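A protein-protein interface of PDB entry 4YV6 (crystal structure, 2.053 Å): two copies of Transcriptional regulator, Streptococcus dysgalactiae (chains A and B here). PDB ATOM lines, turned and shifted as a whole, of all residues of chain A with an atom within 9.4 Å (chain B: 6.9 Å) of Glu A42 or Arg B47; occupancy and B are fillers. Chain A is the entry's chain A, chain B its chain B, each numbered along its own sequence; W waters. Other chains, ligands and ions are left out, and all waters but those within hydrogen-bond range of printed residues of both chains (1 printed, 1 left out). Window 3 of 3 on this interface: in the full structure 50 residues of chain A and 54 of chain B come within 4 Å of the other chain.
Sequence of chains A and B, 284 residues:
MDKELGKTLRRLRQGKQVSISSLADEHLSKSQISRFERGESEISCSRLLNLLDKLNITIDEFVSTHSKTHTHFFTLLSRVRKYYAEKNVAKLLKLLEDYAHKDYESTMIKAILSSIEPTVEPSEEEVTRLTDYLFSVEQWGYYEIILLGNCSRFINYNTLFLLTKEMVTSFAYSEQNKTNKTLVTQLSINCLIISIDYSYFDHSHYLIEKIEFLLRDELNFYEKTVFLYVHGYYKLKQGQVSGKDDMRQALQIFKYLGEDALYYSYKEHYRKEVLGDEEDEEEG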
ATOM      1  N   GLY A   6     -21.548  -2.250   7.056  1.00  0.00           N
ATOM      2  CA  GLY A   6     -21.032  -1.340   8.061  1.00  0.00           C
ATOM      3  C   GLY A   6     -21.030   0.096   7.577  1.00  0.00           C
ATOM      4  O   GLY A   6     -21.409   1.011   8.310  1.00  0.00           O
ATOM      5  N   GLN A  32     -15.638   5.758  18.959  1.00  0.00           N
ATOM      6  CA  GLN A  32     -16.237   4.430  18.977  1.00  0.00           C
ATOM      7  C   GLN A  32     -17.157   4.232  17.777  1.00  0.00           C
ATOM      8  O   GLN A  32     -17.140   3.180  17.143  1.00  0.00           O
ATOM      9  CB  GLN A  32     -17.015   4.209  20.276  1.00  0.00           C
ATOM     10  CG  GLN A  32     -17.672   2.838  20.386  1.00  0.00           C
ATOM     11  CD  GLN A  32     -16.659   1.714  20.466  1.00  0.00           C
ATOM     12  OE1 GLN A  32     -16.184   1.211  19.448  1.00  0.00           O
ATOM     13  NE2 GLN A  32     -16.325   1.313  21.684  1.00  0.00           N
ATOM     14  N   ARG A  35     -15.270   4.061  14.366  1.00  0.00           N
ATOM     15  CA  ARG A  35     -14.990   2.643  14.204  1.00  0.00           C
ATOM     16  C   ARG A  35     -16.315   1.928  13.961  1.00  0.00           C
ATOM     17  O   ARG A  35     -17.322   2.288  14.563  1.00  0.00           O
ATOM     18  CB  ARG A  35     -14.273   2.083  15.435  1.00  0.00           C
ATOM     19  CG  ARG A  35     -12.931   2.751  15.727  1.00  0.00           C
ATOM     20  CD  ARG A  35     -12.244   2.136  16.934  1.00  0.00           C
ATOM     21  NE  ARG A  35     -11.505   3.137  17.708  1.00  0.00           N
ATOM     22  CZ  ARG A  35     -11.644   3.354  19.017  1.00  0.00           C
ATOM     23  NH1 ARG A  35     -12.497   2.642  19.748  1.00  0.00           N
ATOM     24  NH2 ARG A  35     -10.917   4.294  19.607  1.00  0.00           N
ATOM     25  N   PHE A  36     -16.277   0.919  13.088  1.00  0.00           N
ATOM     26  CA  PHE A  36     -17.446   0.259  12.477  1.00  0.00           C
ATOM     27  C   PHE A  36     -17.824   0.983  11.192  1.00  0.00           C
ATOM     28  O   PHE A  36     -17.933   0.360  10.136  1.00  0.00           O
ATOM     29  CB  PHE A  36     -18.670   0.187  13.398  1.00  0.00           C
ATOM     30  CG  PHE A  36     -19.876  -0.407  12.734  1.00  0.00           C
ATOM     31  CD1 PHE A  36     -19.812  -1.651  12.128  1.00  0.00           C
ATOM     32  CD2 PHE A  36     -21.072   0.289  12.701  1.00  0.00           C
ATOM     33  CE1 PHE A  36     -20.923  -2.191  11.506  1.00  0.00           C
ATOM     34  CE2 PHE A  36     -22.181  -0.246  12.086  1.00  0.00           C
ATOM     35  CZ  PHE A  36     -22.109  -1.483  11.483  1.00  0.00           C
ATOM     36  N   GLU A  37     -18.021   2.295  11.273  1.00  0.00           N
ATOM     37  CA  GLU A  37     -18.172   3.093  10.065  1.00  0.00           C
ATOM     38  C   GLU A  37     -16.869   3.031   9.284  1.00  0.00           C
ATOM     39  O   GLU A  37     -16.871   3.053   8.054  1.00  0.00           O
ATOM     40  CB  GLU A  37     -18.534   4.541  10.389  1.00  0.00           C
ATOM     41  CG  GLU A  37     -20.002   4.874  10.171  1.00  0.00           C
ATOM     42  CD  GLU A  37     -20.284   6.362  10.275  1.00  0.00           C
ATOM     43  OE1 GLU A  37     -19.364   7.165  10.012  1.00  0.00           O
ATOM     44  OE2 GLU A  37     -21.426   6.728  10.622  1.00  0.00           O
ATOM     45  N   ARG A  38     -15.759   2.954  10.014  1.00  0.00           N
ATOM     46  CA  ARG A  38     -14.444   2.782   9.407  1.00  0.00           C
ATOM     47  C   ARG A  38     -13.970   1.327   9.500  1.00  0.00           C
ATOM     48  O   ARG A  38     -12.844   1.006   9.125  1.00  0.00           O
ATOM     49  CB  ARG A  38     -13.427   3.722  10.066  1.00  0.00           C
ATOM     50  CG  ARG A  38     -13.113   4.981   9.257  1.00  0.00           C
ATOM     51  CD  ARG A  38     -12.689   4.637   7.836  1.00  0.00           C
ATOM     52  NE  ARG A  38     -11.884   5.686   7.207  1.00  0.00           N
ATOM     53  CZ  ARG A  38     -10.719   5.490   6.589  1.00  0.00           C
ATOM     54  NH1 ARG A  38     -10.183   4.276   6.502  1.00  0.00           N
ATOM     55  NH2 ARG A  38     -10.078   6.518   6.053  1.00  0.00           N
ATOM     56  N   GLY A  39     -14.838   0.455  10.005  1.00  0.00           N
ATOM     57  CA  GLY A  39     -14.616  -0.980   9.950  1.00  0.00           C
ATOM     58  C   GLY A  39     -13.621  -1.525  10.958  1.00  0.00           C
ATOM     59  O   GLY A  39     -13.074  -2.611  10.761  1.00  0.00           O
ATOM     60  N   GLU A  40     -13.395  -0.789  12.041  1.00  0.00           N
ATOM     61  CA  GLU A  40     -12.401  -1.182  13.037  1.00  0.00           C
ATOM     62  C   GLU A  40     -13.014  -1.889  14.246  1.00  0.00           C
ATOM     63  O   GLU A  40     -12.425  -1.884  15.328  1.00  0.00           O
ATOM     64  CB  GLU A  40     -11.626   0.046  13.519  1.00  0.00           C
ATOM     65  CG  GLU A  40     -11.088   0.933  12.406  1.00  0.00           C
ATOM     66  CD  GLU A  40     -10.542   2.246  12.931  1.00  0.00           C
ATOM     67  OE1 GLU A  40     -11.129   3.304  12.616  1.00  0.00           O
ATOM     68  OE2 GLU A  40      -9.527   2.220  13.658  1.00  0.00           O
ATOM     69  N   SER A  41     -14.182  -2.501  14.073  1.00  0.00           N
ATOM     70  CA  SER A  41     -14.856  -3.150  15.198  1.00  0.00           C
ATOM     71  C   SER A  41     -16.073  -3.980  14.803  1.00  0.00           C
ATOM     72  O   SER A  41     -16.815  -3.629  13.884  1.00  0.00           O
ATOM     73  CB  SER A  41     -15.290  -2.097  16.223  1.00  0.00           C
ATOM     74  OG  SER A  41     -14.188  -1.641  16.988  1.00  0.00           O
ATOM     75  N   GLU A  42     -16.260  -5.087  15.514  1.00  0.00           N
ATOM     76  CA  GLU A  42     -17.504  -5.843  15.458  1.00  0.00           C
ATOM     77  C   GLU A  42     -18.599  -5.088  16.195  1.00  0.00           C
ATOM     78  O   GLU A  42     -18.473  -4.828  17.392  1.00  0.00           O
ATOM     79  CB  GLU A  42     -17.339  -7.229  16.086  1.00  0.00           C
ATOM     80  CG  GLU A  42     -16.750  -8.295  15.177  1.00  0.00           C
ATOM     81  CD  GLU A  42     -16.838  -9.687  15.783  1.00  0.00           C
ATOM     82  OE1 GLU A  42     -17.595  -9.871  16.761  1.00  0.00           O
ATOM     83  OE2 GLU A  42     -16.150 -10.599  15.279  1.00  0.00           O
ATOM     84  N   ILE A  43     -19.666  -4.732  15.488  1.00  0.00           N
ATOM     85  CA  ILE A  43     -20.851  -4.194  16.142  1.00  0.00           C
ATOM     86  C   ILE A  43     -21.873  -5.313  16.283  1.00  0.00           C
ATOM     87  O   ILE A  43     -22.079  -6.097  15.357  1.00  0.00           O
ATOM     88  CB  ILE A  43     -21.471  -3.004  15.368  1.00  0.00           C
ATOM     89  CG1 ILE A  43     -22.369  -2.187  16.304  1.00  0.00           C
ATOM     90  CG2 ILE A  43     -22.257  -3.478  14.144  1.00  0.00           C
ATOM     91  CD1 ILE A  43     -22.957  -0.931  15.682  1.00  0.00           C
ATOM     92  N   SER A  44     -22.491  -5.403  17.454  1.00  0.00           N
ATOM     93  CA  SER A  44     -23.592  -6.331  17.653  1.00  0.00           C
ATOM     94  C   SER A  44     -24.843  -5.728  17.029  1.00  0.00           C
ATOM     95  O   SER A  44     -24.973  -4.505  16.952  1.00  0.00           O
ATOM     96  CB  SER A  44     -23.806  -6.615  19.140  1.00  0.00           C
ATOM     97  OG  SER A  44     -24.069  -5.420  19.855  1.00  0.00           O
ATOM     98  N   CYS A  45     -25.757  -6.578  16.572  1.00  0.00           N
ATOM     99  CA  CYS A  45     -26.995  -6.096  15.971  1.00  0.00           C
ATOM    100  C   CYS A  45     -27.779  -5.247  16.964  1.00  0.00           C
ATOM    101  O   CYS A  45     -28.515  -4.342  16.572  1.00  0.00           O
ATOM    102  CB  CYS A  45     -27.853  -7.264  15.484  1.00  0.00           C
ATOM    103  SG  CYS A  45     -27.412  -7.852  13.832  1.00  0.00           S
ATOM    104  N   SER A  46     -27.608  -5.537  18.249  1.00  0.00           N
ATOM    105  CA  SER A  46     -28.262  -4.769  19.299  1.00  0.00           C
ATOM    106  C   SER A  46     -27.831  -3.305  19.243  1.00  0.00           C
ATOM    107  O   SER A  46     -28.659  -2.401  19.350  1.00  0.00           O
ATOM    108  CB  SER A  46     -27.944  -5.361  20.673  1.00  0.00           C
ATOM    109  OG  SER A  46     -28.652  -4.681  21.694  1.00  0.00           O
ATOM    110  N   ARG A  47     -26.534  -3.079  19.064  1.00  0.00           N
ATOM    111  CA  ARG A  47     -25.997  -1.725  19.004  1.00  0.00           C
ATOM    112  C   ARG A  47     -26.247  -1.090  17.639  1.00  0.00           C
ATOM    113  O   ARG A  47     -26.275   0.134  17.516  1.00  0.00           O
ATOM    114  CB  ARG A  47     -24.499  -1.728  19.320  1.00  0.00           C
ATOM    115  CG  ARG A  47     -24.178  -2.139  20.749  1.00  0.00           C
ATOM    116  CD  ARG A  47     -22.700  -1.978  21.066  1.00  0.00           C
ATOM    117  NE  ARG A  47     -22.390  -2.383  22.436  1.00  0.00           N
ATOM    118  CZ  ARG A  47     -22.576  -1.617  23.508  1.00  0.00           C
ATOM    119  NH1 ARG A  47     -23.077  -0.393  23.384  1.00  0.00           N
ATOM    120  NH2 ARG A  47     -22.262  -2.075  24.712  1.00  0.00           N
ATOM    121  N   LEU A  48     -26.428  -1.920  16.616  1.00  0.00           N
ATOM    122  CA  LEU A  48     -26.739  -1.415  15.284  1.00  0.00           C
ATOM    123  C   LEU A  48     -28.168  -0.888  15.242  1.00  0.00           C
ATOM    124  O   LEU A  48     -28.415   0.211  14.747  1.00  0.00           O
ATOM    125  CB  LEU A  48     -26.547  -2.503  14.225  1.00  0.00           C
ATOM    126  CG  LEU A  48     -26.975  -2.116  12.804  1.00  0.00           C
ATOM    127  CD1 LEU A  48     -26.276  -0.840  12.342  1.00  0.00           C
ATOM    128  CD2 LEU A  48     -26.699  -3.252  11.834  1.00  0.00           C
ATOM    129  N   GLU B  26     -16.735 -20.891   7.771  1.00  0.00           N
ATOM    130  CA  GLU B  26     -15.476 -20.186   7.983  1.00  0.00           C
ATOM    131  C   GLU B  26     -15.565 -19.084   9.043  1.00  0.00           C
ATOM    132  O   GLU B  26     -14.568 -18.758   9.687  1.00  0.00           O
ATOM    133  CB  GLU B  26     -15.017 -19.583   6.655  1.00  0.00           C
ATOM    134  CG  GLU B  26     -13.573 -19.132   6.618  1.00  0.00           C
ATOM    135  CD  GLU B  26     -13.168 -18.633   5.244  1.00  0.00           C
ATOM    136  OE1 GLU B  26     -14.068 -18.261   4.458  1.00  0.00           O
ATOM    137  OE2 GLU B  26     -11.954 -18.619   4.947  1.00  0.00           O
ATOM    138  N   HIS B  27     -16.758 -18.522   9.225  1.00  0.00           N
ATOM    139  CA  HIS B  27     -16.930 -17.330  10.055  1.00  0.00           C
ATOM    140  C   HIS B  27     -17.434 -17.645  11.462  1.00  0.00           C
ATOM    141  O   HIS B  27     -17.041 -16.985  12.424  1.00  0.00           O
ATOM    142  CB  HIS B  27     -17.889 -16.359   9.368  1.00  0.00           C
ATOM    143  CG  HIS B  27     -17.560 -16.110   7.929  1.00  0.00           C
ATOM    144  ND1 HIS B  27     -18.204 -16.754   6.896  1.00  0.00           N
ATOM    145  CD2 HIS B  27     -16.638 -15.301   7.355  1.00  0.00           C
ATOM    146  CE1 HIS B  27     -17.701 -16.344   5.743  1.00  0.00           C
ATOM    147  NE2 HIS B  27     -16.751 -15.463   5.995  1.00  0.00           N
ATOM    148  N   LEU B  28     -18.307 -18.643  11.575  1.00  0.00           N
ATOM    149  CA  LEU B  28     -18.826 -19.069  12.872  1.00  0.00           C
ATOM    150  C   LEU B  28     -18.808 -20.584  13.009  1.00  0.00           C
ATOM    151  O   LEU B  28     -19.324 -21.300  12.153  1.00  0.00           O
ATOM    152  CB  LEU B  28     -20.257 -18.555  13.085  1.00  0.00           C
ATOM    153  CG  LEU B  28     -20.450 -17.141  13.637  1.00  0.00           C
ATOM    154  CD1 LEU B  28     -21.937 -16.834  13.753  1.00  0.00           C
ATOM    155  CD2 LEU B  28     -19.775 -16.963  14.991  1.00  0.00           C
ATOM    156  N   GLN B  32     -19.704 -21.592  18.536  1.00  0.00           N
ATOM    157  CA  GLN B  32     -19.978 -20.161  18.615  1.00  0.00           C
ATOM    158  C   GLN B  32     -21.453 -19.861  18.356  1.00  0.00           C
ATOM    159  O   GLN B  32     -22.000 -18.891  18.881  1.00  0.00           O
ATOM    160  CB  GLN B  32     -19.098 -19.397  17.623  1.00  0.00           C
ATOM    161  CG  GLN B  32     -17.635 -19.312  18.044  1.00  0.00           C
ATOM    162  CD  GLN B  32     -16.745 -18.708  16.974  1.00  0.00           C
ATOM    163  OE1 GLN B  32     -17.013 -18.834  15.779  1.00  0.00           O
ATOM    164  NE2 GLN B  32     -15.678 -18.044  17.401  1.00  0.00           N
ATOM    165  N   GLU B  42     -21.714 -13.332  22.468  1.00  0.00           N
ATOM    166  CA  GLU B  42     -22.316 -12.418  21.503  1.00  0.00           C
ATOM    167  C   GLU B  42     -21.521 -12.408  20.203  1.00  0.00           C
ATOM    168  O   GLU B  42     -20.292 -12.478  20.213  1.00  0.00           O
ATOM    169  CB  GLU B  42     -22.402 -11.003  22.077  1.00  0.00           C
ATOM    170  CG  GLU B  42     -23.503 -10.828  23.111  1.00  0.00           C
ATOM    171  CD  GLU B  42     -23.665  -9.386  23.555  1.00  0.00           C
ATOM    172  OE1 GLU B  42     -22.863  -8.533  23.117  1.00  0.00           O
ATOM    173  OE2 GLU B  42     -24.597  -9.105  24.339  1.00  0.00           O
ATOM    174  N   ILE B  43     -22.242 -12.322  19.089  1.00  0.00           N
ATOM    175  CA  ILE B  43     -21.638 -12.316  17.762  1.00  0.00           C
ATOM    176  C   ILE B  43     -21.880 -10.982  17.066  1.00  0.00           C
ATOM    177  O   ILE B  43     -22.761 -10.216  17.460  1.00  0.00           O
ATOM    178  CB  ILE B  43     -22.197 -13.456  16.887  1.00  0.00           C
ATOM    179  CG1 ILE B  43     -23.728 -13.367  16.809  1.00  0.00           C
ATOM    180  CG2 ILE B  43     -21.758 -14.806  17.444  1.00  0.00           C
ATOM    181  CD1 ILE B  43     -24.358 -14.326  15.823  1.00  0.00           C
ATOM    182  N   SER B  44     -21.091 -10.710  16.033  1.00  0.00           N
ATOM    183  CA  SER B  44     -21.262  -9.502  15.238  1.00  0.00           C
ATOM    184  C   SER B  44     -22.566  -9.566  14.465  1.00  0.00           C
ATOM    185  O   SER B  44     -23.135 -10.641  14.274  1.00  0.00           O
ATOM    186  CB  SER B  44     -20.097  -9.320  14.268  1.00  0.00           C
ATOM    187  OG  SER B  44     -20.017 -10.416  13.375  1.00  0.00           O
ATOM    188  N   CYS B  45     -23.032  -8.411  14.008  1.00  0.00           N
ATOM    189  CA  CYS B  45     -24.246  -8.359  13.214  1.00  0.00           C
ATOM    190  C   CYS B  45     -23.988  -8.981  11.848  1.00  0.00           C
ATOM    191  O   CYS B  45     -24.857  -9.642  11.284  1.00  0.00           O
ATOM    192  CB  CYS B  45     -24.735  -6.919  13.067  1.00  0.00           C
ATOM    193  SG  CYS B  45     -26.418  -6.772  12.426  1.00  0.00           S
ATOM    194  N   SER B  46     -22.781  -8.774  11.330  1.00  0.00           N
ATOM    195  CA  SER B  46     -22.386  -9.338  10.045  1.00  0.00           C
ATOM    196  C   SER B  46     -22.487 -10.860  10.066  1.00  0.00           C
ATOM    197  O   SER B  46     -22.909 -11.478   9.090  1.00  0.00           O
ATOM    198  CB  SER B  46     -20.959  -8.918   9.687  1.00  0.00           C
ATOM    199  OG  SER B  46     -20.838  -7.508   9.630  1.00  0.00           O
ATOM    200  N   ARG B  47     -22.100 -11.456  11.190  1.00  0.00           N
ATOM    201  CA  ARG B  47     -22.120 -12.906  11.332  1.00  0.00           C
ATOM    202  C   ARG B  47     -23.537 -13.427  11.572  1.00  0.00           C
ATOM    203  O   ARG B  47     -23.875 -14.529  11.142  1.00  0.00           O
ATOM    204  CB  ARG B  47     -21.192 -13.341  12.468  1.00  0.00           C
ATOM    205  CG  ARG B  47     -19.717 -13.318  12.090  1.00  0.00           C
ATOM    206  CD  ARG B  47     -18.829 -13.749  13.245  1.00  0.00           C
ATOM    207  NE  ARG B  47     -17.470 -14.053  12.804  1.00  0.00           N
ATOM    208  CZ  ARG B  47     -16.496 -13.156  12.680  1.00  0.00           C
ATOM    209  NH1 ARG B  47     -16.714 -11.876  12.960  1.00  0.00           N
ATOM    210  NH2 ARG B  47     -15.294 -13.539  12.270  1.00  0.00           N
ATOM    211  N   LEU B  48     -24.361 -12.639  12.257  1.00  0.00           N
ATOM    212  CA  LEU B  48     -25.765 -12.994  12.436  1.00  0.00           C
ATOM    213  C   LEU B  48     -26.470 -12.993  11.085  1.00  0.00           C
ATOM    214  O   LEU B  48     -27.193 -13.930  10.754  1.00  0.00           O
ATOM    215  CB  LEU B  48     -26.461 -12.027  13.398  1.00  0.00           C
ATOM    216  CG  LEU B  48     -27.966 -12.250  13.598  1.00  0.00           C
ATOM    217  CD1 LEU B  48     -28.259 -13.666  14.071  1.00  0.00           C
ATOM    218  CD2 LEU B  48     -28.532 -11.242  14.581  1.00  0.00           C
ATOM    219  N   LEU B  49     -26.247 -11.935  10.312  1.00  0.00           N
ATOM    220  CA  LEU B  49     -26.831 -11.812   8.981  1.00  0.00           C
ATOM    221  C   LEU B  49     -26.424 -12.969   8.078  1.00  0.00           C
ATOM    222  O   LEU B  49     -27.197 -13.395   7.220  1.00  0.00           O
ATOM    223  CB  LEU B  49     -26.422 -10.483   8.343  1.00  0.00           C
ATOM    224  CG  LEU B  49     -27.411  -9.325   8.516  1.00  0.00           C
ATOM    225  CD1 LEU B  49     -27.884  -9.188   9.956  1.00  0.00           C
ATOM    226  CD2 LEU B  49     -26.783  -8.022   8.044  1.00  0.00           C
ATOM    227  N   ASN B  50     -25.210 -13.473   8.271  1.00  0.00           N
ATOM    228  CA  ASN B  50     -24.741 -14.628   7.518  1.00  0.00           C
ATOM    229  C   ASN B  50     -25.580 -15.858   7.853  1.00  0.00           C
ATOM    230  O   ASN B  50     -25.992 -16.601   6.962  1.00  0.00           O
ATOM    231  CB  ASN B  50     -23.262 -14.897   7.812  1.00  0.00           C
ATOM    232  CG  ASN B  50     -22.682 -16.001   6.945  1.00  0.00           C
ATOM    233  OD1 ASN B  50     -22.990 -16.103   5.758  1.00  0.00           O
ATOM    234  ND2 ASN B  50     -21.838 -16.837   7.538  1.00  0.00           N
ATOM    235  N   LEU B  51     -25.837 -16.063   9.142  1.00  0.00           N
ATOM    236  CA  LEU B  51     -26.659 -17.180   9.596  1.00  0.00           C
ATOM    237  C   LEU B  51     -28.078 -17.069   9.057  1.00  0.00           C
ATOM    238  O   LEU B  51     -28.652 -18.049   8.582  1.00  0.00           O
ATOM    239  CB  LEU B  51     -26.698 -17.237  11.123  1.00  0.00           C
ATOM    240  CG  LEU B  51     -25.375 -17.513  11.834  1.00  0.00           C
ATOM    241  CD1 LEU B  51     -25.549 -17.365  13.341  1.00  0.00           C
ATOM    242  CD2 LEU B  51     -24.855 -18.898  11.485  1.00  0.00           C
ATOM    243  N   LEU B  52     -28.642 -15.869   9.145  1.00  0.00           N
ATOM    244  CA  LEU B  52     -30.006 -15.629   8.699  1.00  0.00           C
ATOM    245  C   LEU B  52     -30.126 -15.814   7.188  1.00  0.00           C
ATOM    246  O   LEU B  52     -31.149 -16.290   6.695  1.00  0.00           O
ATOM    247  CB  LEU B  52     -30.455 -14.223   9.099  1.00  0.00           C
ATOM    248  CG  LEU B  52     -30.487 -13.913  10.596  1.00  0.00           C
ATOM    249  CD1 LEU B  52     -30.889 -12.466  10.817  1.00  0.00           C
ATOM    250  CD2 LEU B  52     -31.436 -14.853  11.324  1.00  0.00           C
HETATM  251  O   HOH W   1     -21.262  -6.536  12.248  1.00  0.00           O
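The side-chain carboxylate (OE2) of Glu A42 lies within salt-bridge range of the guanidinium group (NH1) of Arg B47, 2.7 Å away. O of Ile A43 is in hydrogen-bond range of N of Cys B45 (2.8 Å). The side-chain sulfur of Cys A45 forms a disulfide with the side-chain sulfur of Cys B45, 2.0 Å away.
The backbone NH of Arg A47 sits close to the side-chain hydroxyl of Ser A44 (3.5 Å). The guanidinium group (NE) of Arg B47 is in hydrogen-bond range of the backbone carbonyl oxygen (O) of His B27, at 3.0 Å. The side-chain hydroxyl (OG) of Ser B44 lies close to the backbone NH (N) of Arg B47 (3.2 Å).
Among the printed residues, merely in contact across the chains: Glu A42 with Ser B44, Ile A43 with Ser B44, Ser A44 with Ile B43, Cys A45 with Leu B48 and Leu A48 with Cys B45.
Glu A40 touches none of the printed residues of chain B. Of the printed residues of chain B, Glu A42 touches Ser B44 (3.6 Å) and Arg B47 (2.7 Å). Printed residues of chain B within 4 Å of Ile A43: Ser B44 and Cys B45. Printed residues of chain B within 4 Å of Ser A44: Ile B43. Of the printed residues of chain B, Cys A45 touches Cys B45 and Leu B48. Of the printed residues of chain B, Leu A48 touches Cys B45 (3.6 Å). Leu B28 touches none of the printed residues of chain A. Ser B44 touches just these residues of chain A: Glu A42 (3.6 Å) and Ile A43 (3.5 Å). Of chain A, only Glu A42 (2.7 Å) comes within 4 Å of Arg B47. Of the printed residues of chain A, Leu B48 touches Cys A45 (3.6 Å). The nearest residue of chain A that does not touch Arg B47 is Ile A43 (6.8 Å). The nearest printed residue of chain B that does not touch Ile A43 is Ile B43 (4.7 Å).
Of the 16 printed residues of chain A, 5 touch a printed residue of chain B. Printed residues of chain A that touch a printed residue of chain B: Glu A42, Ile A43, Ser A44, Cys A45 and Leu A48. Hydrophobic or aromatic side chains of chain A within 4 Å of the printed part of chain B: Leu A48. Printed residues of chain B that touch a printed residue of chain A: Ile B43, Ser B44, Cys B45, Arg B47 and Leu B48. Among the printed residues, 8 pairs touch across the chains. Among the printed residues, Asp or Glu carboxylates within 4 Å of a Lys or Arg side-chain nitrogen of the other chain: Glu A42 with Arg B47.
Glu A42 touches Arg B47, but with the chains exchanged Arg A47 does not touch Glu B42 (6.2 Å). Ile A43 touches Cys B45, but with the chains exchanged Cys A45 does not touch Ile B43 (4.8 Å). Cys B45 touches its own counterpart, Cys A45. Cys A45 touches Leu B48, and with the chains exchanged Leu A48 touches Cys B45. Of the 8 pairs that touch across the chains among the printed residues, 5 have their exchanged pair printed and touching as well.
Water W1 lies within hydrogen-bond range of the side-chain hydroxyl of Ser B46 (2.8 Å), the backbone NH of Cys B45 (3.1 Å) and the backbone carbonyl oxygen of Ile A43 (3.2 Å).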
